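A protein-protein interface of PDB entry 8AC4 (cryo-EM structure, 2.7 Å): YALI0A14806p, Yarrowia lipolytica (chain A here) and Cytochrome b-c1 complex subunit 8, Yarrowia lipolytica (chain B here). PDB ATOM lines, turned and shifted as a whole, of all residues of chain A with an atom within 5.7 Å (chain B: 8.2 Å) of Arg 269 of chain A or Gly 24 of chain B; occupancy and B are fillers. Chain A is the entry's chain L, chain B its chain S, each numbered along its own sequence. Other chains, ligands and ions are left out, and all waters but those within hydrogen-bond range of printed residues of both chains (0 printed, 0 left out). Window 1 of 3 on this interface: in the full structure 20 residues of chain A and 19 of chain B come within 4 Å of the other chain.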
ATOM      1  N   GLU A 267     -12.384 -15.302  32.440  1.00  0.00           N
ATOM      2  CA  GLU A 267     -11.211 -14.467  32.616  1.00  0.00           C
ATOM      3  C   GLU A 267     -11.575 -13.199  33.352  1.00  0.00           C
ATOM      4  O   GLU A 267     -12.708 -12.732  33.271  1.00  0.00           O
ATOM      5  CB  GLU A 267     -10.527 -14.051  31.323  1.00  0.00           C
ATOM      6  CG  GLU A 267     -11.518 -13.869  30.236  1.00  0.00           C
ATOM      7  CD  GLU A 267     -10.927 -13.097  29.077  1.00  0.00           C
ATOM      8  OE1 GLU A 267      -9.984 -13.614  28.438  1.00  0.00           O
ATOM      9  OE2 GLU A 267     -11.412 -11.979  28.811  1.00  0.00           O
ATOM     10  N   VAL A 268     -10.579 -12.679  34.060  1.00  0.00           N
ATOM     11  CA  VAL A 268     -10.655 -11.376  34.674  1.00  0.00           C
ATOM     12  C   VAL A 268      -9.480 -10.598  34.122  1.00  0.00           C
ATOM     13  O   VAL A 268      -8.351 -11.060  34.236  1.00  0.00           O
ATOM     14  CB  VAL A 268     -10.522 -11.476  36.198  1.00  0.00           C
ATOM     15  CG1 VAL A 268     -10.606 -10.100  36.822  1.00  0.00           C
ATOM     16  CG2 VAL A 268     -11.551 -12.412  36.804  1.00  0.00           C
ATOM     17  N   ARG A 269      -9.748  -9.428  33.550  1.00  0.00           N
ATOM     18  CA  ARG A 269      -8.650  -8.573  33.146  1.00  0.00           C
ATOM     19  C   ARG A 269      -8.643  -7.331  34.018  1.00  0.00           C
ATOM     20  O   ARG A 269      -9.657  -6.650  34.143  1.00  0.00           O
ATOM     21  CB  ARG A 269      -8.799  -8.157  31.693  1.00  0.00           C
ATOM     22  CG  ARG A 269      -8.820  -9.337  30.740  1.00  0.00           C
ATOM     23  CD  ARG A 269      -9.242  -8.782  29.407  1.00  0.00           C
ATOM     24  NE  ARG A 269      -8.097  -9.133  28.604  1.00  0.00           N
ATOM     25  CZ  ARG A 269      -7.945 -10.229  27.879  1.00  0.00           C
ATOM     26  NH1 ARG A 269      -8.897 -11.133  27.715  1.00  0.00           N
ATOM     27  NH2 ARG A 269      -6.800 -10.365  27.259  1.00  0.00           N
ATOM     28  N   LEU A 270      -7.488  -7.042  34.609  1.00  0.00           N
ATOM     29  CA  LEU A 270      -7.359  -5.888  35.469  1.00  0.00           C
ATOM     30  C   LEU A 270      -6.262  -5.048  34.849  1.00  0.00           C
ATOM     31  O   LEU A 270      -5.140  -4.995  35.349  1.00  0.00           O
ATOM     32  CB  LEU A 270      -6.971  -6.372  36.868  1.00  0.00           C
ATOM     33  CG  LEU A 270      -7.908  -7.397  37.504  1.00  0.00           C
ATOM     34  CD1 LEU A 270      -7.226  -8.132  38.656  1.00  0.00           C
ATOM     35  CD2 LEU A 270      -9.179  -6.732  38.007  1.00  0.00           C
ATOM     36  N   ARG A 271      -6.580  -4.476  33.698  1.00  0.00           N
ATOM     37  CA  ARG A 271      -5.563  -3.737  32.989  1.00  0.00           C
ATOM     38  C   ARG A 271      -5.181  -2.478  33.761  1.00  0.00           C
ATOM     39  O   ARG A 271      -6.044  -1.776  34.279  1.00  0.00           O
ATOM     40  CB  ARG A 271      -6.079  -3.388  31.603  1.00  0.00           C
ATOM     41  CG  ARG A 271      -5.140  -2.476  30.843  1.00  0.00           C
ATOM     42  CD  ARG A 271      -5.520  -2.735  29.421  1.00  0.00           C
ATOM     43  NE  ARG A 271      -4.893  -1.664  28.680  1.00  0.00           N
ATOM     44  CZ  ARG A 271      -5.108  -1.424  27.397  1.00  0.00           C
ATOM     45  NH1 ARG A 271      -5.961  -2.168  26.710  1.00  0.00           N
ATOM     46  NH2 ARG A 271      -4.491  -0.412  26.820  1.00  0.00           N
ATOM     47  N   LEU A 450      -8.372 -17.441  33.611  1.00  0.00           N
ATOM     48  CA  LEU A 450      -7.256 -16.632  33.178  1.00  0.00           C
ATOM     49  C   LEU A 450      -7.369 -15.294  33.883  1.00  0.00           C
ATOM     50  O   LEU A 450      -8.434 -14.696  33.908  1.00  0.00           O
ATOM     51  CB  LEU A 450      -7.417 -16.485  31.670  1.00  0.00           C
ATOM     52  CG  LEU A 450      -6.646 -15.333  31.048  1.00  0.00           C
ATOM     53  CD1 LEU A 450      -5.177 -15.674  30.944  1.00  0.00           C
ATOM     54  CD2 LEU A 450      -7.180 -15.066  29.657  1.00  0.00           C
ATOM     55  N   VAL A 451      -6.291 -14.832  34.494  1.00  0.00           N
ATOM     56  CA  VAL A 451      -6.356 -13.541  35.142  1.00  0.00           C
ATOM     57  C   VAL A 451      -5.150 -12.770  34.671  1.00  0.00           C
ATOM     58  O   VAL A 451      -4.049 -13.297  34.731  1.00  0.00           O
ATOM     59  CB  VAL A 451      -6.286 -13.668  36.664  1.00  0.00           C
ATOM     60  CG1 VAL A 451      -6.178 -12.284  37.276  1.00  0.00           C
ATOM     61  CG2 VAL A 451      -7.477 -14.414  37.225  1.00  0.00           C
ATOM     62  N   GLY A 452      -5.367 -11.551  34.200  1.00  0.00           N
ATOM     63  CA  GLY A 452      -4.245 -10.724  33.809  1.00  0.00           C
ATOM     64  C   GLY A 452      -4.310  -9.414  34.570  1.00  0.00           C
ATOM     65  O   GLY A 452      -5.382  -8.836  34.718  1.00  0.00           O
ATOM     66  N   ILE A 456      -1.623  -5.366  30.024  1.00  0.00           N
ATOM     67  CA  ILE A 456      -1.947  -6.632  29.390  1.00  0.00           C
ATOM     68  C   ILE A 456      -2.732  -6.379  28.106  1.00  0.00           C
ATOM     69  O   ILE A 456      -3.452  -7.262  27.647  1.00  0.00           O
ATOM     70  CB  ILE A 456      -2.755  -7.495  30.370  1.00  0.00           C
ATOM     71  CG1 ILE A 456      -3.951  -6.684  30.879  1.00  0.00           C
ATOM     72  CG2 ILE A 456      -1.861  -7.978  31.502  1.00  0.00           C
ATOM     73  CD1 ILE A 456      -5.052  -7.483  31.534  1.00  0.00           C
ATOM     74  N   LEU A 459      -2.428  -9.102  25.711  1.00  0.00           N
ATOM     75  CA  LEU A 459      -2.966 -10.418  25.988  1.00  0.00           C
ATOM     76  C   LEU A 459      -4.227 -10.547  25.147  1.00  0.00           C
ATOM     77  O   LEU A 459      -5.073  -9.671  25.222  1.00  0.00           O
ATOM     78  CB  LEU A 459      -3.268 -10.459  27.484  1.00  0.00           C
ATOM     79  CG  LEU A 459      -3.913 -11.742  27.990  1.00  0.00           C
ATOM     80  CD1 LEU A 459      -2.943 -12.899  27.872  1.00  0.00           C
ATOM     81  CD2 LEU A 459      -4.354 -11.577  29.436  1.00  0.00           C
ATOM     82  N   TYR A 460      -4.307 -11.556  24.272  1.00  0.00           N
ATOM     83  CA  TYR A 460      -5.476 -11.662  23.406  1.00  0.00           C
ATOM     84  C   TYR A 460      -6.707 -12.049  24.210  1.00  0.00           C
ATOM     85  O   TYR A 460      -6.599 -12.415  25.375  1.00  0.00           O
ATOM     86  CB  TYR A 460      -5.275 -12.710  22.316  1.00  0.00           C
ATOM     87  CG  TYR A 460      -4.225 -12.319  21.314  1.00  0.00           C
ATOM     88  CD1 TYR A 460      -4.116 -11.004  20.881  1.00  0.00           C
ATOM     89  CD2 TYR A 460      -3.320 -13.249  20.827  1.00  0.00           C
ATOM     90  CE1 TYR A 460      -3.140 -10.623  19.978  1.00  0.00           C
ATOM     91  CE2 TYR A 460      -2.342 -12.886  19.911  1.00  0.00           C
ATOM     92  CZ  TYR A 460      -2.249 -11.567  19.491  1.00  0.00           C
ATOM     93  OH  TYR A 460      -1.299 -11.179  18.595  1.00  0.00           O
ATOM     94  N   ASP A 461      -7.863 -11.977  23.561  1.00  0.00           N
ATOM     95  CA  ASP A 461      -9.147 -12.319  24.145  1.00  0.00           C
ATOM     96  C   ASP A 461      -9.202 -13.805  24.517  1.00  0.00           C
ATOM     97  O   ASP A 461      -8.363 -14.619  24.114  1.00  0.00           O
ATOM     98  CB  ASP A 461     -10.219 -11.936  23.128  1.00  0.00           C
ATOM     99  CG  ASP A 461      -9.808 -12.398  21.737  1.00  0.00           C
ATOM    100  OD1 ASP A 461      -9.706 -13.624  21.562  1.00  0.00           O
ATOM    101  OD2 ASP A 461      -9.551 -11.531  20.855  1.00  0.00           O
ATOM    102  N   TYR A 462     -10.234 -14.158  25.283  1.00  0.00           N
ATOM    103  CA  TYR A 462     -10.352 -15.502  25.808  1.00  0.00           C
ATOM    104  C   TYR A 462     -10.250 -16.558  24.707  1.00  0.00           C
ATOM    105  O   TYR A 462      -9.542 -17.528  24.908  1.00  0.00           O
ATOM    106  CB  TYR A 462     -11.626 -15.644  26.629  1.00  0.00           C
ATOM    107  CG  TYR A 462     -11.698 -16.955  27.358  1.00  0.00           C
ATOM    108  CD1 TYR A 462     -12.246 -18.080  26.753  1.00  0.00           C
ATOM    109  CD2 TYR A 462     -11.217 -17.086  28.657  1.00  0.00           C
ATOM    110  CE1 TYR A 462     -12.318 -19.296  27.421  1.00  0.00           C
ATOM    111  CE2 TYR A 462     -11.282 -18.299  29.336  1.00  0.00           C
ATOM    112  CZ  TYR A 462     -11.816 -19.418  28.709  1.00  0.00           C
ATOM    113  OH  TYR A 462     -11.871 -20.627  29.359  1.00  0.00           O
ATOM    114  N   TRP B  11      -0.798  -4.614  18.987  1.00  0.00           N
ATOM    115  CA  TRP B  11      -1.013  -5.159  20.312  1.00  0.00           C
ATOM    116  C   TRP B  11       0.159  -4.821  21.217  1.00  0.00           C
ATOM    117  O   TRP B  11       1.314  -5.055  20.863  1.00  0.00           O
ATOM    118  CB  TRP B  11      -1.120  -6.661  20.184  1.00  0.00           C
ATOM    119  CG  TRP B  11      -2.226  -7.039  19.266  1.00  0.00           C
ATOM    120  CD1 TRP B  11      -2.124  -7.461  17.974  1.00  0.00           C
ATOM    121  CD2 TRP B  11      -3.623  -7.003  19.585  1.00  0.00           C
ATOM    122  NE1 TRP B  11      -3.371  -7.716  17.476  1.00  0.00           N
ATOM    123  CE2 TRP B  11      -4.309  -7.443  18.434  1.00  0.00           C
ATOM    124  CE3 TRP B  11      -4.351  -6.639  20.725  1.00  0.00           C
ATOM    125  CZ2 TRP B  11      -5.698  -7.527  18.390  1.00  0.00           C
ATOM    126  CZ3 TRP B  11      -5.725  -6.732  20.684  1.00  0.00           C
ATOM    127  CH2 TRP B  11      -6.385  -7.163  19.529  1.00  0.00           C
ATOM    128  N   GLY B  21      -8.272   1.008  36.388  1.00  0.00           N
ATOM    129  CA  GLY B  21      -9.498   1.013  37.160  1.00  0.00           C
ATOM    130  C   GLY B  21     -10.652   0.247  36.522  1.00  0.00           C
ATOM    131  O   GLY B  21     -11.692   0.105  37.157  1.00  0.00           O
ATOM    132  N   ILE B  22     -10.482  -0.304  35.316  1.00  0.00           N
ATOM    133  CA  ILE B  22     -11.569  -1.092  34.756  1.00  0.00           C
ATOM    134  C   ILE B  22     -11.267  -2.576  34.935  1.00  0.00           C
ATOM    135  O   ILE B  22     -10.226  -3.039  34.480  1.00  0.00           O
ATOM    136  CB  ILE B  22     -11.769  -0.746  33.274  1.00  0.00           C
ATOM    137  CG1 ILE B  22     -11.965   0.755  33.054  1.00  0.00           C
ATOM    138  CG2 ILE B  22     -12.911  -1.560  32.688  1.00  0.00           C
ATOM    139  CD1 ILE B  22     -11.732   1.193  31.621  1.00  0.00           C
ATOM    140  N   ALA B  23     -12.182  -3.325  35.562  1.00  0.00           N
ATOM    141  CA  ALA B  23     -12.053  -4.772  35.623  1.00  0.00           C
ATOM    142  C   ALA B  23     -13.005  -5.361  34.592  1.00  0.00           C
ATOM    143  O   ALA B  23     -14.169  -4.974  34.562  1.00  0.00           O
ATOM    144  CB  ALA B  23     -12.382  -5.262  37.009  1.00  0.00           C
ATOM    145  N   GLY B  24     -12.509  -6.260  33.742  1.00  0.00           N
ATOM    146  CA  GLY B  24     -13.367  -6.882  32.748  1.00  0.00           C
ATOM    147  C   GLY B  24     -13.558  -8.352  33.077  1.00  0.00           C
ATOM    148  O   GLY B  24     -12.616  -9.011  33.498  1.00  0.00           O
ATOM    149  N   TYR B  25     -14.765  -8.863  32.876  1.00  0.00           N
ATOM    150  CA  TYR B  25     -15.012 -10.248  33.210  1.00  0.00           C
ATOM    151  C   TYR B  25     -15.752 -10.910  32.074  1.00  0.00           C
ATOM    152  O   TYR B  25     -16.638 -10.302  31.490  1.00  0.00           O
ATOM    153  CB  TYR B  25     -15.989 -10.315  34.372  1.00  0.00           C
ATOM    154  CG  TYR B  25     -15.438  -9.644  35.589  1.00  0.00           C
ATOM    155  CD1 TYR B  25     -15.499  -8.264  35.733  1.00  0.00           C
ATOM    156  CD2 TYR B  25     -14.846 -10.394  36.593  1.00  0.00           C
ATOM    157  CE1 TYR B  25     -14.994  -7.645  36.861  1.00  0.00           C
ATOM    158  CE2 TYR B  25     -14.321  -9.791  37.721  1.00  0.00           C
ATOM    159  CZ  TYR B  25     -14.405  -8.418  37.853  1.00  0.00           C
ATOM    160  OH  TYR B  25     -13.896  -7.840  38.970  1.00  0.00           O
ATOM    161  N   THR B  26     -15.414 -12.167  31.792  1.00  0.00           N
ATOM    162  CA  THR B  26     -16.227 -12.902  30.845  1.00  0.00           C
ATOM    163  C   THR B  26     -16.131 -14.402  31.073  1.00  0.00           C
ATOM    164  O   THR B  26     -15.239 -14.873  31.756  1.00  0.00           O
ATOM    165  CB  THR B  26     -15.872 -12.537  29.403  1.00  0.00           C
ATOM    166  OG1 THR B  26     -16.966 -13.068  28.654  1.00  0.00           O
ATOM    167  CG2 THR B  26     -14.551 -13.115  28.957  1.00  0.00           C
ATOM    168  N   ILE B  27     -17.029 -15.155  30.452  1.00  0.00           N
ATOM    169  CA  ILE B  27     -16.972 -16.596  30.612  1.00  0.00           C
ATOM    170  C   ILE B  27     -16.708 -17.263  29.267  1.00  0.00           C
ATOM    171  O   ILE B  27     -16.993 -16.699  28.213  1.00  0.00           O
ATOM    172  CB  ILE B  27     -18.249 -17.107  31.294  1.00  0.00           C
ATOM    173  CG1 ILE B  27     -19.478 -16.757  30.451  1.00  0.00           C
ATOM    174  CG2 ILE B  27     -18.332 -16.553  32.712  1.00  0.00           C
ATOM    175  CD1 ILE B  27     -20.748 -17.439  30.885  1.00  0.00           C
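The backbone NH (N) of Glu 267 of chain A sits at hydrogen-bond distance from the backbone carbonyl oxygen (O) of Thr 26 of chain B (3.0 Å).
N of Arg 269 of chain A sits at hydrogen-bond distance from O of Gly 24 of chain B.
OE1 of Glu 267 of chain A lies within salt-bridge range of NH1 of Arg 269 of chain A, at 2.8 Å.
The backbone carbonyl oxygen (O) of Leu 450 of chain A sits at hydrogen-bond distance from the backbone NH (N) of Val 268 of chain A, at 2.9 Å.
The backbone carbonyl oxygen of Val 268 of chain A lies within hydrogen-bond range of the backbone NH of Gly 452 of chain A, at 3.0 Å.
The guanidinium group (NH2) of Arg 269 of chain A is in hydrogen-bond range of the backbone carbonyl oxygen (O) of Leu 459 of chain A, at 2.8 Å.
The backbone carbonyl oxygen (O) of Tyr 460 of chain A lies within hydrogen-bond range of the guanidinium group (NH2) of Arg 269 of chain A, 2.8 Å away.
The backbone carbonyl oxygen (O) of Gly 452 of chain A lies within hydrogen-bond range of the backbone NH (N) of Leu 270 of chain A.
Among the printed residues, merely in contact across the chains: Val 268 of chain A with Gly 24 of chain B, Arg 269 of chain A with Ala 23 of chain B, Glu 267 of chain A with Tyr 25 of chain B, Leu 270 of chain A with Ala 23 of chain B, Arg 269 of chain A with Ile 22 of chain B, Tyr 460 of chain A with Trp 11 of chain B, Glu 267 of chain A with Gly 24 of chain B, Val 268 of chain A with Tyr 25 of chain B and Arg 271 of chain A with Ile 22 of chain B.
Printed residues of chain B within 4 Å of Arg 269 of chain A: Ile 22, Ala 23 and Gly 24.
Leu 459 of chain A touches none of the printed residues of chain B.
Printed residues of chain B within 4 Å of Tyr 460 of chain A: Trp 11.
Of chain A, only Glu 267 (3.7 Å), Val 268 (3.3 Å) and Arg 269 (2.9 Å) come within 4 Å of Gly 24 of chain B.
Printed residues of chain A within 4 Å of Tyr 25 of chain B: Glu 267 and Val 268.
Ile 27 of chain B touches none of the printed residues of chain A.
The nearest residue of chain B that does not touch Arg 269 of chain A is Tyr 25 of chain B (5.1 Å).
The nearest printed residue of chain B that does not touch Leu 270 of chain A is Ile 22 of chain B (4.2 Å).
Of the 13 printed residues of chain A, 6 touch a printed residue of chain B.
Hydrophobic or aromatic side chains of chain A that line the printed part of chain B: Val 268, Leu 270 and Tyr 460.
Of the 8 printed residues of chain B, 6 touch a printed residue of chain A.
Printed residues of chain B that touch a printed residue of chain A: Trp 11, Ile 22, Ala 23, Gly 24, Tyr 25 and Thr 26.
Hydrophobic or aromatic side chains of chain B within 4 Å of the printed part of chain A: Trp 11, Ala 23 and Tyr 25.
Among the printed residues, no Asp or Glu carboxylate lies within 4 Å of a Lys or Arg side-chain nitrogen of the other chain.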
